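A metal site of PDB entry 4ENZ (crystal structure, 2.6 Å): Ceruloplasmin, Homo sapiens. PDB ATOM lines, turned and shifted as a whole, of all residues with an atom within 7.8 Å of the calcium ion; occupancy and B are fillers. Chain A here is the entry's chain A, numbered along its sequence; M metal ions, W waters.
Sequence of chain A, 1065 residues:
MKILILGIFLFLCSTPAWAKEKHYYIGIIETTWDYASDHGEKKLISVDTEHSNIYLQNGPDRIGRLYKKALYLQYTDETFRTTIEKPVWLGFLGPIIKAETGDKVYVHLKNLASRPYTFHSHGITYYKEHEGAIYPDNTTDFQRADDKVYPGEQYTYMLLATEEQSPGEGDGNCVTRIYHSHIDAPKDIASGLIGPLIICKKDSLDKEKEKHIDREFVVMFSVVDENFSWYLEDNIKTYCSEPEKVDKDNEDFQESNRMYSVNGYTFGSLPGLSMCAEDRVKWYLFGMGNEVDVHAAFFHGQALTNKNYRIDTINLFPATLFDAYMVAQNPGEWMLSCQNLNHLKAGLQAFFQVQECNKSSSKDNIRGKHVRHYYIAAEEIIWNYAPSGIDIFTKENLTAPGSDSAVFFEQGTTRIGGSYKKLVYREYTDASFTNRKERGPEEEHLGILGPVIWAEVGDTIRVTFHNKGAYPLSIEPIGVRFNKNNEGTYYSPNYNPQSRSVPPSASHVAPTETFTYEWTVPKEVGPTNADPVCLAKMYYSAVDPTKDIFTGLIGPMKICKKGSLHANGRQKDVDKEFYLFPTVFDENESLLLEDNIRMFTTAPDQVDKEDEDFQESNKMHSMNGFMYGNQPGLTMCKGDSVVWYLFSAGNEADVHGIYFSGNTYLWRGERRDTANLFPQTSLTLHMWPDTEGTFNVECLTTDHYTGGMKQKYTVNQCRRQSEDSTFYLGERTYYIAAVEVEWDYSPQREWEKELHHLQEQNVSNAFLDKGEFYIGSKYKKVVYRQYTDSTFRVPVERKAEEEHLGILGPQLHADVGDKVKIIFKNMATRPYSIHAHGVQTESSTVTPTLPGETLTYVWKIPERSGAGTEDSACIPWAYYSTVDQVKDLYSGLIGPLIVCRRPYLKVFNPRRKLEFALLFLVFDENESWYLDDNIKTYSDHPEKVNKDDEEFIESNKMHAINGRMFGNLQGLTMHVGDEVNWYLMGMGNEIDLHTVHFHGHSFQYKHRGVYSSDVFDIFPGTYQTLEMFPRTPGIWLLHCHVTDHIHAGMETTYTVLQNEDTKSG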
ATOM      1  N   TYR A 127      -4.359 -24.026 -10.165  1.00  0.00           N
ATOM      2  CA  TYR A 127      -4.223 -24.333  -8.736  1.00  0.00           C
ATOM      3  C   TYR A 127      -4.964 -25.646  -8.419  1.00  0.00           C
ATOM      4  O   TYR A 127      -5.687 -26.179  -9.262  1.00  0.00           O
ATOM      5  CB  TYR A 127      -4.749 -23.195  -7.903  1.00  0.00           C
ATOM      6  CG  TYR A 127      -4.087 -21.839  -8.118  1.00  0.00           C
ATOM      7  CD1 TYR A 127      -4.847 -20.721  -8.492  1.00  0.00           C
ATOM      8  CD2 TYR A 127      -2.715 -21.659  -7.889  1.00  0.00           C
ATOM      9  CE1 TYR A 127      -4.253 -19.479  -8.670  1.00  0.00           C
ATOM     10  CE2 TYR A 127      -2.113 -20.421  -8.044  1.00  0.00           C
ATOM     11  CZ  TYR A 127      -2.884 -19.342  -8.438  1.00  0.00           C
ATOM     12  OH  TYR A 127      -2.312 -18.108  -8.596  1.00  0.00           O
ATOM     13  N   LYS A 128      -4.824 -26.156  -7.208  1.00  0.00           N
ATOM     14  CA  LYS A 128      -5.545 -27.379  -6.818  1.00  0.00           C
ATOM     15  C   LYS A 128      -7.085 -27.289  -6.912  1.00  0.00           C
ATOM     16  O   LYS A 128      -7.729 -28.320  -7.130  1.00  0.00           O
ATOM     17  CB  LYS A 128      -5.130 -27.831  -5.421  1.00  0.00           C
ATOM     18  CG  LYS A 128      -3.680 -28.224  -5.291  1.00  0.00           C
ATOM     19  CD  LYS A 128      -3.395 -29.472  -6.093  1.00  0.00           C
ATOM     20  CE  LYS A 128      -3.878 -30.705  -5.352  1.00  0.00           C
ATOM     21  NZ  LYS A 128      -3.490 -31.971  -6.040  1.00  0.00           N
ATOM     22  N   GLU A 129      -7.658 -26.085  -6.777  1.00  0.00           N
ATOM     23  CA  GLU A 129      -9.085 -25.854  -6.977  1.00  0.00           C
ATOM     24  C   GLU A 129      -9.542 -26.140  -8.373  1.00  0.00           C
ATOM     25  O   GLU A 129     -10.742 -26.098  -8.629  1.00  0.00           O
ATOM     26  CB  GLU A 129      -9.502 -24.359  -6.812  1.00  0.00           C
ATOM     27  CG  GLU A 129      -9.052 -23.614  -5.621  1.00  0.00           C
ATOM     28  CD  GLU A 129      -7.664 -23.074  -5.757  1.00  0.00           C
ATOM     29  OE1 GLU A 129      -7.472 -21.848  -5.953  1.00  0.00           O
ATOM     30  OE2 GLU A 129      -6.746 -23.904  -5.653  1.00  0.00           O
ATOM     31  N   HIS A 130      -8.621 -26.244  -9.318  1.00  0.00           N
ATOM     32  CA  HIS A 130      -8.990 -26.298 -10.730  1.00  0.00           C
ATOM     33  C   HIS A 130      -8.366 -27.446 -11.507  1.00  0.00           C
ATOM     34  O   HIS A 130      -8.360 -27.433 -12.715  1.00  0.00           O
ATOM     35  CB  HIS A 130      -8.693 -24.967 -11.387  1.00  0.00           C
ATOM     36  CG  HIS A 130      -9.396 -23.795 -10.758  1.00  0.00           C
ATOM     37  ND1 HIS A 130      -8.723 -22.731 -10.189  1.00  0.00           N
ATOM     38  CD2 HIS A 130     -10.712 -23.528 -10.618  1.00  0.00           C
ATOM     39  CE1 HIS A 130      -9.606 -21.860  -9.727  1.00  0.00           C
ATOM     40  NE2 HIS A 130     -10.813 -22.307  -9.985  1.00  0.00           N
ATOM     41  N   GLU A 131      -7.884 -28.446 -10.798  1.00  0.00           N
ATOM     42  CA  GLU A 131      -7.255 -29.631 -11.385  1.00  0.00           C
ATOM     43  C   GLU A 131      -8.281 -30.656 -11.850  1.00  0.00           C
ATOM     44  O   GLU A 131      -8.027 -31.435 -12.732  1.00  0.00           O
ATOM     45  CB  GLU A 131      -6.353 -30.306 -10.310  1.00  0.00           C
ATOM     46  CG  GLU A 131      -5.599 -31.570 -10.718  1.00  0.00           C
ATOM     47  CD  GLU A 131      -4.763 -32.145  -9.560  1.00  0.00           C
ATOM     48  OE1 GLU A 131      -4.943 -31.726  -8.381  1.00  0.00           O
ATOM     49  OE2 GLU A 131      -3.935 -33.048  -9.840  1.00  0.00           O
ATOM     50  N   GLY A 132      -9.422 -30.705 -11.197  1.00  0.00           N
ATOM     51  CA  GLY A 132     -10.444 -31.652 -11.611  1.00  0.00           C
ATOM     52  C   GLY A 132     -10.065 -33.107 -11.484  1.00  0.00           C
ATOM     53  O   GLY A 132     -10.443 -33.926 -12.295  1.00  0.00           O
ATOM     54  N   ALA A 133      -9.342 -33.452 -10.444  1.00  0.00           N
ATOM     55  CA  ALA A 133      -8.939 -34.827 -10.264  1.00  0.00           C
ATOM     56  C   ALA A 133      -8.900 -35.154  -8.758  1.00  0.00           C
ATOM     57  O   ALA A 133      -8.404 -34.370  -7.950  1.00  0.00           O
ATOM     58  CB  ALA A 133      -7.599 -35.073 -10.931  1.00  0.00           C
ATOM     59  N   ILE A 134      -9.455 -36.315  -8.397  1.00  0.00           N
ATOM     60  CA  ILE A 134      -9.618 -36.691  -7.019  1.00  0.00           C
ATOM     61  C   ILE A 134      -8.569 -37.704  -6.641  1.00  0.00           C
ATOM     62  O   ILE A 134      -8.338 -38.662  -7.345  1.00  0.00           O
ATOM     63  CB  ILE A 134     -11.032 -37.239  -6.721  1.00  0.00           C
ATOM     64  CG1 ILE A 134     -11.440 -36.930  -5.253  1.00  0.00           C
ATOM     65  CG2 ILE A 134     -11.110 -38.730  -7.017  1.00  0.00           C
ATOM     66  CD1 ILE A 134     -12.924 -36.834  -5.018  1.00  0.00           C
ATOM     67  N   TYR A 135      -7.893 -37.452  -5.537  1.00  0.00           N
ATOM     68  CA  TYR A 135      -6.854 -38.354  -5.041  1.00  0.00           C
ATOM     69  C   TYR A 135      -6.284 -37.777  -3.771  1.00  0.00           C
ATOM     70  O   TYR A 135      -6.463 -36.578  -3.516  1.00  0.00           O
ATOM     71  CB  TYR A 135      -5.726 -38.559  -6.059  1.00  0.00           C
ATOM     72  CG  TYR A 135      -4.975 -37.320  -6.554  1.00  0.00           C
ATOM     73  CD1 TYR A 135      -5.301 -36.735  -7.751  1.00  0.00           C
ATOM     74  CD2 TYR A 135      -3.890 -36.794  -5.853  1.00  0.00           C
ATOM     75  CE1 TYR A 135      -4.568 -35.643  -8.250  1.00  0.00           C
ATOM     76  CE2 TYR A 135      -3.162 -35.686  -6.325  1.00  0.00           C
ATOM     77  CZ  TYR A 135      -3.503 -35.126  -7.529  1.00  0.00           C
ATOM     78  OH  TYR A 135      -2.804 -34.068  -8.043  1.00  0.00           O
ATOM     79  N   ASP A 137      -4.266 -35.876  -1.574  1.00  0.00           N
ATOM     80  CA  ASP A 137      -3.327 -34.784  -1.726  1.00  0.00           C
ATOM     81  C   ASP A 137      -3.375 -33.746  -0.570  1.00  0.00           C
ATOM     82  O   ASP A 137      -2.827 -32.628  -0.707  1.00  0.00           O
ATOM     83  CB  ASP A 137      -3.686 -34.088  -3.051  1.00  0.00           C
ATOM     84  CG  ASP A 137      -5.095 -33.505  -3.064  1.00  0.00           C
ATOM     85  OD1 ASP A 137      -5.743 -33.407  -2.000  1.00  0.00           O
ATOM     86  OD2 ASP A 137      -5.564 -33.135  -4.139  1.00  0.00           O
ATOM     87  N   THR A 139      -5.791 -31.876   0.536  1.00  0.00           N
ATOM     88  CA  THR A 139      -6.479 -30.616   0.252  1.00  0.00           C
ATOM     89  C   THR A 139      -7.739 -30.531   1.057  1.00  0.00           C
ATOM     90  O   THR A 139      -8.214 -31.520   1.571  1.00  0.00           O
ATOM     91  CB  THR A 139      -6.802 -30.442  -1.246  1.00  0.00           C
ATOM     92  OG1 THR A 139      -7.247 -31.674  -1.802  1.00  0.00           O
ATOM     93  CG2 THR A 139      -5.599 -29.985  -2.005  1.00  0.00           C
ATOM     94  N   THR A 140      -8.277 -29.319   1.146  1.00  0.00           N
ATOM     95  CA  THR A 140      -9.402 -29.003   1.983  1.00  0.00           C
ATOM     96  C   THR A 140     -10.619 -28.811   1.112  1.00  0.00           C
ATOM     97  O   THR A 140     -10.479 -28.731  -0.107  1.00  0.00           O
ATOM     98  CB  THR A 140      -9.006 -27.797   2.843  1.00  0.00           C
ATOM     99  OG1 THR A 140      -8.451 -28.298   4.054  1.00  0.00           O
ATOM    100  CG2 THR A 140     -10.158 -26.883   3.190  1.00  0.00           C
ATOM    101  N   ASP A 141     -11.808 -28.773   1.709  1.00  0.00           N
ATOM    102  CA  ASP A 141     -13.054 -28.609   0.958  1.00  0.00           C
ATOM    103  C   ASP A 141     -12.995 -27.623  -0.213  1.00  0.00           C
ATOM    104  O   ASP A 141     -13.596 -27.879  -1.258  1.00  0.00           O
ATOM    105  CB  ASP A 141     -14.194 -28.173   1.869  1.00  0.00           C
ATOM    106  CG  ASP A 141     -14.554 -29.222   2.902  1.00  0.00           C
ATOM    107  OD1 ASP A 141     -14.739 -30.376   2.471  1.00  0.00           O
ATOM    108  OD2 ASP A 141     -14.645 -28.893   4.135  1.00  0.00           O
ATOM    109  N   PHE A 142     -12.318 -26.493  -0.057  1.00  0.00           N
ATOM    110  CA  PHE A 142     -12.373 -25.459  -1.096  1.00  0.00           C
ATOM    111  C   PHE A 142     -11.479 -25.815  -2.287  1.00  0.00           C
ATOM    112  O   PHE A 142     -11.601 -25.200  -3.334  1.00  0.00           O
ATOM    113  CB  PHE A 142     -12.088 -24.035  -0.548  1.00  0.00           C
ATOM    114  CG  PHE A 142     -10.614 -23.709  -0.433  1.00  0.00           C
ATOM    115  CD1 PHE A 142      -9.811 -24.302   0.594  1.00  0.00           C
ATOM    116  CD2 PHE A 142      -9.992 -22.856  -1.361  1.00  0.00           C
ATOM    117  CE1 PHE A 142      -8.417 -24.051   0.712  1.00  0.00           C
ATOM    118  CE2 PHE A 142      -8.583 -22.574  -1.243  1.00  0.00           C
ATOM    119  CZ  PHE A 142      -7.809 -23.191  -0.196  1.00  0.00           C
ATOM    120  N   GLN A 143     -10.584 -26.794  -2.138  1.00  0.00           N
ATOM    121  CA  GLN A 143      -9.706 -27.224  -3.260  1.00  0.00           C
ATOM    122  C   GLN A 143     -10.167 -28.551  -3.816  1.00  0.00           C
ATOM    123  O   GLN A 143      -9.538 -29.115  -4.707  1.00  0.00           O
ATOM    124  CB  GLN A 143      -8.266 -27.320  -2.806  1.00  0.00           C
ATOM    125  CG  GLN A 143      -7.617 -25.983  -2.492  1.00  0.00           C
ATOM    126  CD  GLN A 143      -6.337 -26.145  -1.687  1.00  0.00           C
ATOM    127  OE1 GLN A 143      -6.335 -26.729  -0.600  1.00  0.00           O
ATOM    128  NE2 GLN A 143      -5.249 -25.624  -2.222  1.00  0.00           N
ATOM    129  N   ARG A 144     -11.294 -29.013  -3.284  1.00  0.00           N
ATOM    130  CA  ARG A 144     -11.886 -30.314  -3.608  1.00  0.00           C
ATOM    131  C   ARG A 144     -13.206 -30.208  -4.342  1.00  0.00           C
ATOM    132  O   ARG A 144     -13.695 -31.203  -4.830  1.00  0.00           O
ATOM    133  CB  ARG A 144     -12.132 -31.104  -2.298  1.00  0.00           C
ATOM    134  CG  ARG A 144     -10.993 -32.027  -1.938  1.00  0.00           C
ATOM    135  CD  ARG A 144     -11.038 -33.301  -2.756  1.00  0.00           C
ATOM    136  NE  ARG A 144      -9.803 -34.104  -2.610  1.00  0.00           N
ATOM    137  CZ  ARG A 144      -9.514 -34.835  -1.533  1.00  0.00           C
ATOM    138  NH1 ARG A 144     -10.365 -34.862  -0.489  1.00  0.00           N
ATOM    139  NH2 ARG A 144      -8.375 -35.533  -1.492  1.00  0.00           N
ATOM    140  N   ALA A 145     -13.808 -29.033  -4.372  1.00  0.00           N
ATOM    141  CA  ALA A 145     -15.115 -28.855  -5.046  1.00  0.00           C
ATOM    142  C   ALA A 145     -14.934 -29.222  -6.494  1.00  0.00           C
ATOM    143  O   ALA A 145     -15.828 -29.805  -7.102  1.00  0.00           O
ATOM    144  CB  ALA A 145     -15.615 -27.455  -4.919  1.00  0.00           C
ATOM    145  N   ASP A 146     -13.751 -28.925  -7.034  1.00  0.00           N
ATOM    146  CA  ASP A 146     -13.423 -29.223  -8.427  1.00  0.00           C
ATOM    147  C   ASP A 146     -13.322 -30.704  -8.795  1.00  0.00           C
ATOM    148  O   ASP A 146     -13.356 -31.046  -9.985  1.00  0.00           O
ATOM    149  CB  ASP A 146     -12.113 -28.521  -8.829  1.00  0.00           C
ATOM    150  CG  ASP A 146     -10.900 -29.052  -8.108  1.00  0.00           C
ATOM    151  OD1 ASP A 146     -10.926 -29.275  -6.891  1.00  0.00           O
ATOM    152  OD2 ASP A 146      -9.881 -29.199  -8.766  1.00  0.00           O
ATOM    153  N   ASP A 147     -13.250 -31.560  -7.791  1.00  0.00           N
ATOM    154  CA  ASP A 147     -12.792 -32.907  -7.977  1.00  0.00           C
ATOM    155  C   ASP A 147     -13.929 -33.915  -8.000  1.00  0.00           C
ATOM    156  O   ASP A 147     -13.702 -35.099  -8.164  1.00  0.00           O
ATOM    157  CB  ASP A 147     -11.814 -33.250  -6.850  1.00  0.00           C
ATOM    158  CG  ASP A 147     -10.549 -32.379  -6.880  1.00  0.00           C
ATOM    159  OD1 ASP A 147     -10.241 -31.784  -7.937  1.00  0.00           O
ATOM    160  OD2 ASP A 147      -9.849 -32.310  -5.836  1.00  0.00           O
ATOM    161  N   LYS A 148     -15.157 -33.447  -7.838  1.00  0.00           N
ATOM    162  CA  LYS A 148     -16.318 -34.312  -7.832  1.00  0.00           C
ATOM    163  C   LYS A 148     -17.561 -33.431  -8.108  1.00  0.00           C
ATOM    164  O   LYS A 148     -18.185 -32.915  -7.192  1.00  0.00           O
ATOM    165  CB  LYS A 148     -16.432 -35.046  -6.504  1.00  0.00           C
ATOM    166  CG  LYS A 148     -17.287 -36.296  -6.535  1.00  0.00           C
ATOM    167  CD  LYS A 148     -17.914 -36.623  -5.161  1.00  0.00           C
ATOM    168  CE  LYS A 148     -17.623 -38.068  -4.608  1.00  0.00           C
ATOM    169  NZ  LYS A 148     -16.179 -38.385  -4.349  1.00  0.00           N
ATOM    170  N   TYR A 155     -19.423 -26.201 -12.106  1.00  0.00           N
ATOM    171  CA  TYR A 155     -18.145 -25.687 -11.574  1.00  0.00           C
ATOM    172  C   TYR A 155     -17.376 -25.056 -12.701  1.00  0.00           C
ATOM    173  O   TYR A 155     -17.405 -25.536 -13.835  1.00  0.00           O
ATOM    174  CB  TYR A 155     -17.289 -26.797 -10.975  1.00  0.00           C
ATOM    175  CG  TYR A 155     -16.097 -26.298 -10.181  1.00  0.00           C
ATOM    176  CD1 TYR A 155     -14.896 -25.934 -10.796  1.00  0.00           C
ATOM    177  CD2 TYR A 155     -16.173 -26.180  -8.799  1.00  0.00           C
ATOM    178  CE1 TYR A 155     -13.823 -25.485 -10.054  1.00  0.00           C
ATOM    179  CE2 TYR A 155     -15.112 -25.725  -8.052  1.00  0.00           C
ATOM    180  CZ  TYR A 155     -13.948 -25.382  -8.670  1.00  0.00           C
ATOM    181  OH  TYR A 155     -12.906 -24.968  -7.879  1.00  0.00           O
ATOM    182  N   TYR A 157     -13.796 -23.819 -14.061  1.00  0.00           N
ATOM    183  CA  TYR A 157     -12.397 -24.018 -13.925  1.00  0.00           C
ATOM    184  C   TYR A 157     -11.558 -22.878 -14.529  1.00  0.00           C
ATOM    185  O   TYR A 157     -11.811 -22.485 -15.666  1.00  0.00           O
ATOM    186  CB  TYR A 157     -12.072 -25.298 -14.677  1.00  0.00           C
ATOM    187  CG  TYR A 157     -12.603 -26.575 -14.088  1.00  0.00           C
ATOM    188  CD1 TYR A 157     -13.914 -26.961 -14.306  1.00  0.00           C
ATOM    189  CD2 TYR A 157     -11.781 -27.425 -13.351  1.00  0.00           C
ATOM    190  CE1 TYR A 157     -14.386 -28.167 -13.802  1.00  0.00           C
ATOM    191  CE2 TYR A 157     -12.235 -28.601 -12.862  1.00  0.00           C
ATOM    192  CZ  TYR A 157     -13.541 -28.957 -13.082  1.00  0.00           C
ATOM    193  OH  TYR A 157     -14.020 -30.133 -12.553  1.00  0.00           O
ATOM    194  N   TRP A1036       0.873 -33.324  -6.026  1.00  0.00           N
ATOM    195  CA  TRP A1036       0.421 -33.624  -7.356  1.00  0.00           C
ATOM    196  C   TRP A1036       0.689 -35.061  -7.729  1.00  0.00           C
ATOM    197  O   TRP A1036       1.733 -35.600  -7.413  1.00  0.00           O
ATOM    198  CB  TRP A1036       1.201 -32.769  -8.336  1.00  0.00           C
ATOM    199  CG  TRP A1036       1.096 -31.349  -8.134  1.00  0.00           C
ATOM    200  CD1 TRP A1036       2.033 -30.549  -7.568  1.00  0.00           C
ATOM    201  CD2 TRP A1036       0.036 -30.518  -8.519  1.00  0.00           C
ATOM    202  NE1 TRP A1036       1.628 -29.260  -7.599  1.00  0.00           N
ATOM    203  CE2 TRP A1036       0.393 -29.214  -8.188  1.00  0.00           C
ATOM    204  CE3 TRP A1036      -1.172 -30.740  -9.175  1.00  0.00           C
ATOM    205  CZ2 TRP A1036      -0.437 -28.122  -8.439  1.00  0.00           C
ATOM    206  CZ3 TRP A1036      -1.988 -29.668  -9.430  1.00  0.00           C
ATOM    207  CH2 TRP A1036      -1.623 -28.374  -9.068  1.00  0.00           C
HETATM  208 CA    CA M   1      -8.789 -30.234  -6.501  1.00  0.00          CA
HETATM  209  O   HOH W   1      -7.530 -31.920  -7.512  1.00  0.00           O
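The side-chain carboxylate of Glu 131 is in salt-bridge range of the side-chain amino group of Lys 128, at 2.8 Å. NZ of Lys 128 lies within salt-bridge range of OD2 of Asp 137 (3.0 Å). The side-chain amino group (NZ) of Lys 128 is in hydrogen-bond range of the side-chain hydroxyl (OH) of Tyr 135, 3.0 Å away. The side-chain carboxylate (OD2) of Asp 146 sits close to the backbone NH (N) of Glu 131. The side-chain carboxylate (OD2) of Asp 146 sits close to the backbone NH (N) of Gly 132 (2.9 Å). N of His 130 lies close to OD2 of Asp 146 (3.3 Å). The side-chain hydroxyl (OH) of Tyr 157 lies within hydrogen-bond range of the backbone carbonyl oxygen (O) of Asp 146, at 2.8 Å. OD2 of Asp 147 sits close to NE of Arg 144 (3.7 Å).
Of the 23 residues printed, 4 come within 4 Å of the calcium ion.
The calcium ion is bound by O of Gln 143 (2.2 Å), O of Lys 128 (2.3 Å), water W1 (2.3 Å), OD1 of Asp 146 (2.4 Å), OD2 of Asp 147 (2.4 Å), OD1 of Asp 147 (2.6 Å) and OD2 of Asp 146 (2.7 Å).
Water W1 bridges O of Ala 133 (2.6 Å) and OE1 of Glu 131 (2.7 Å).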
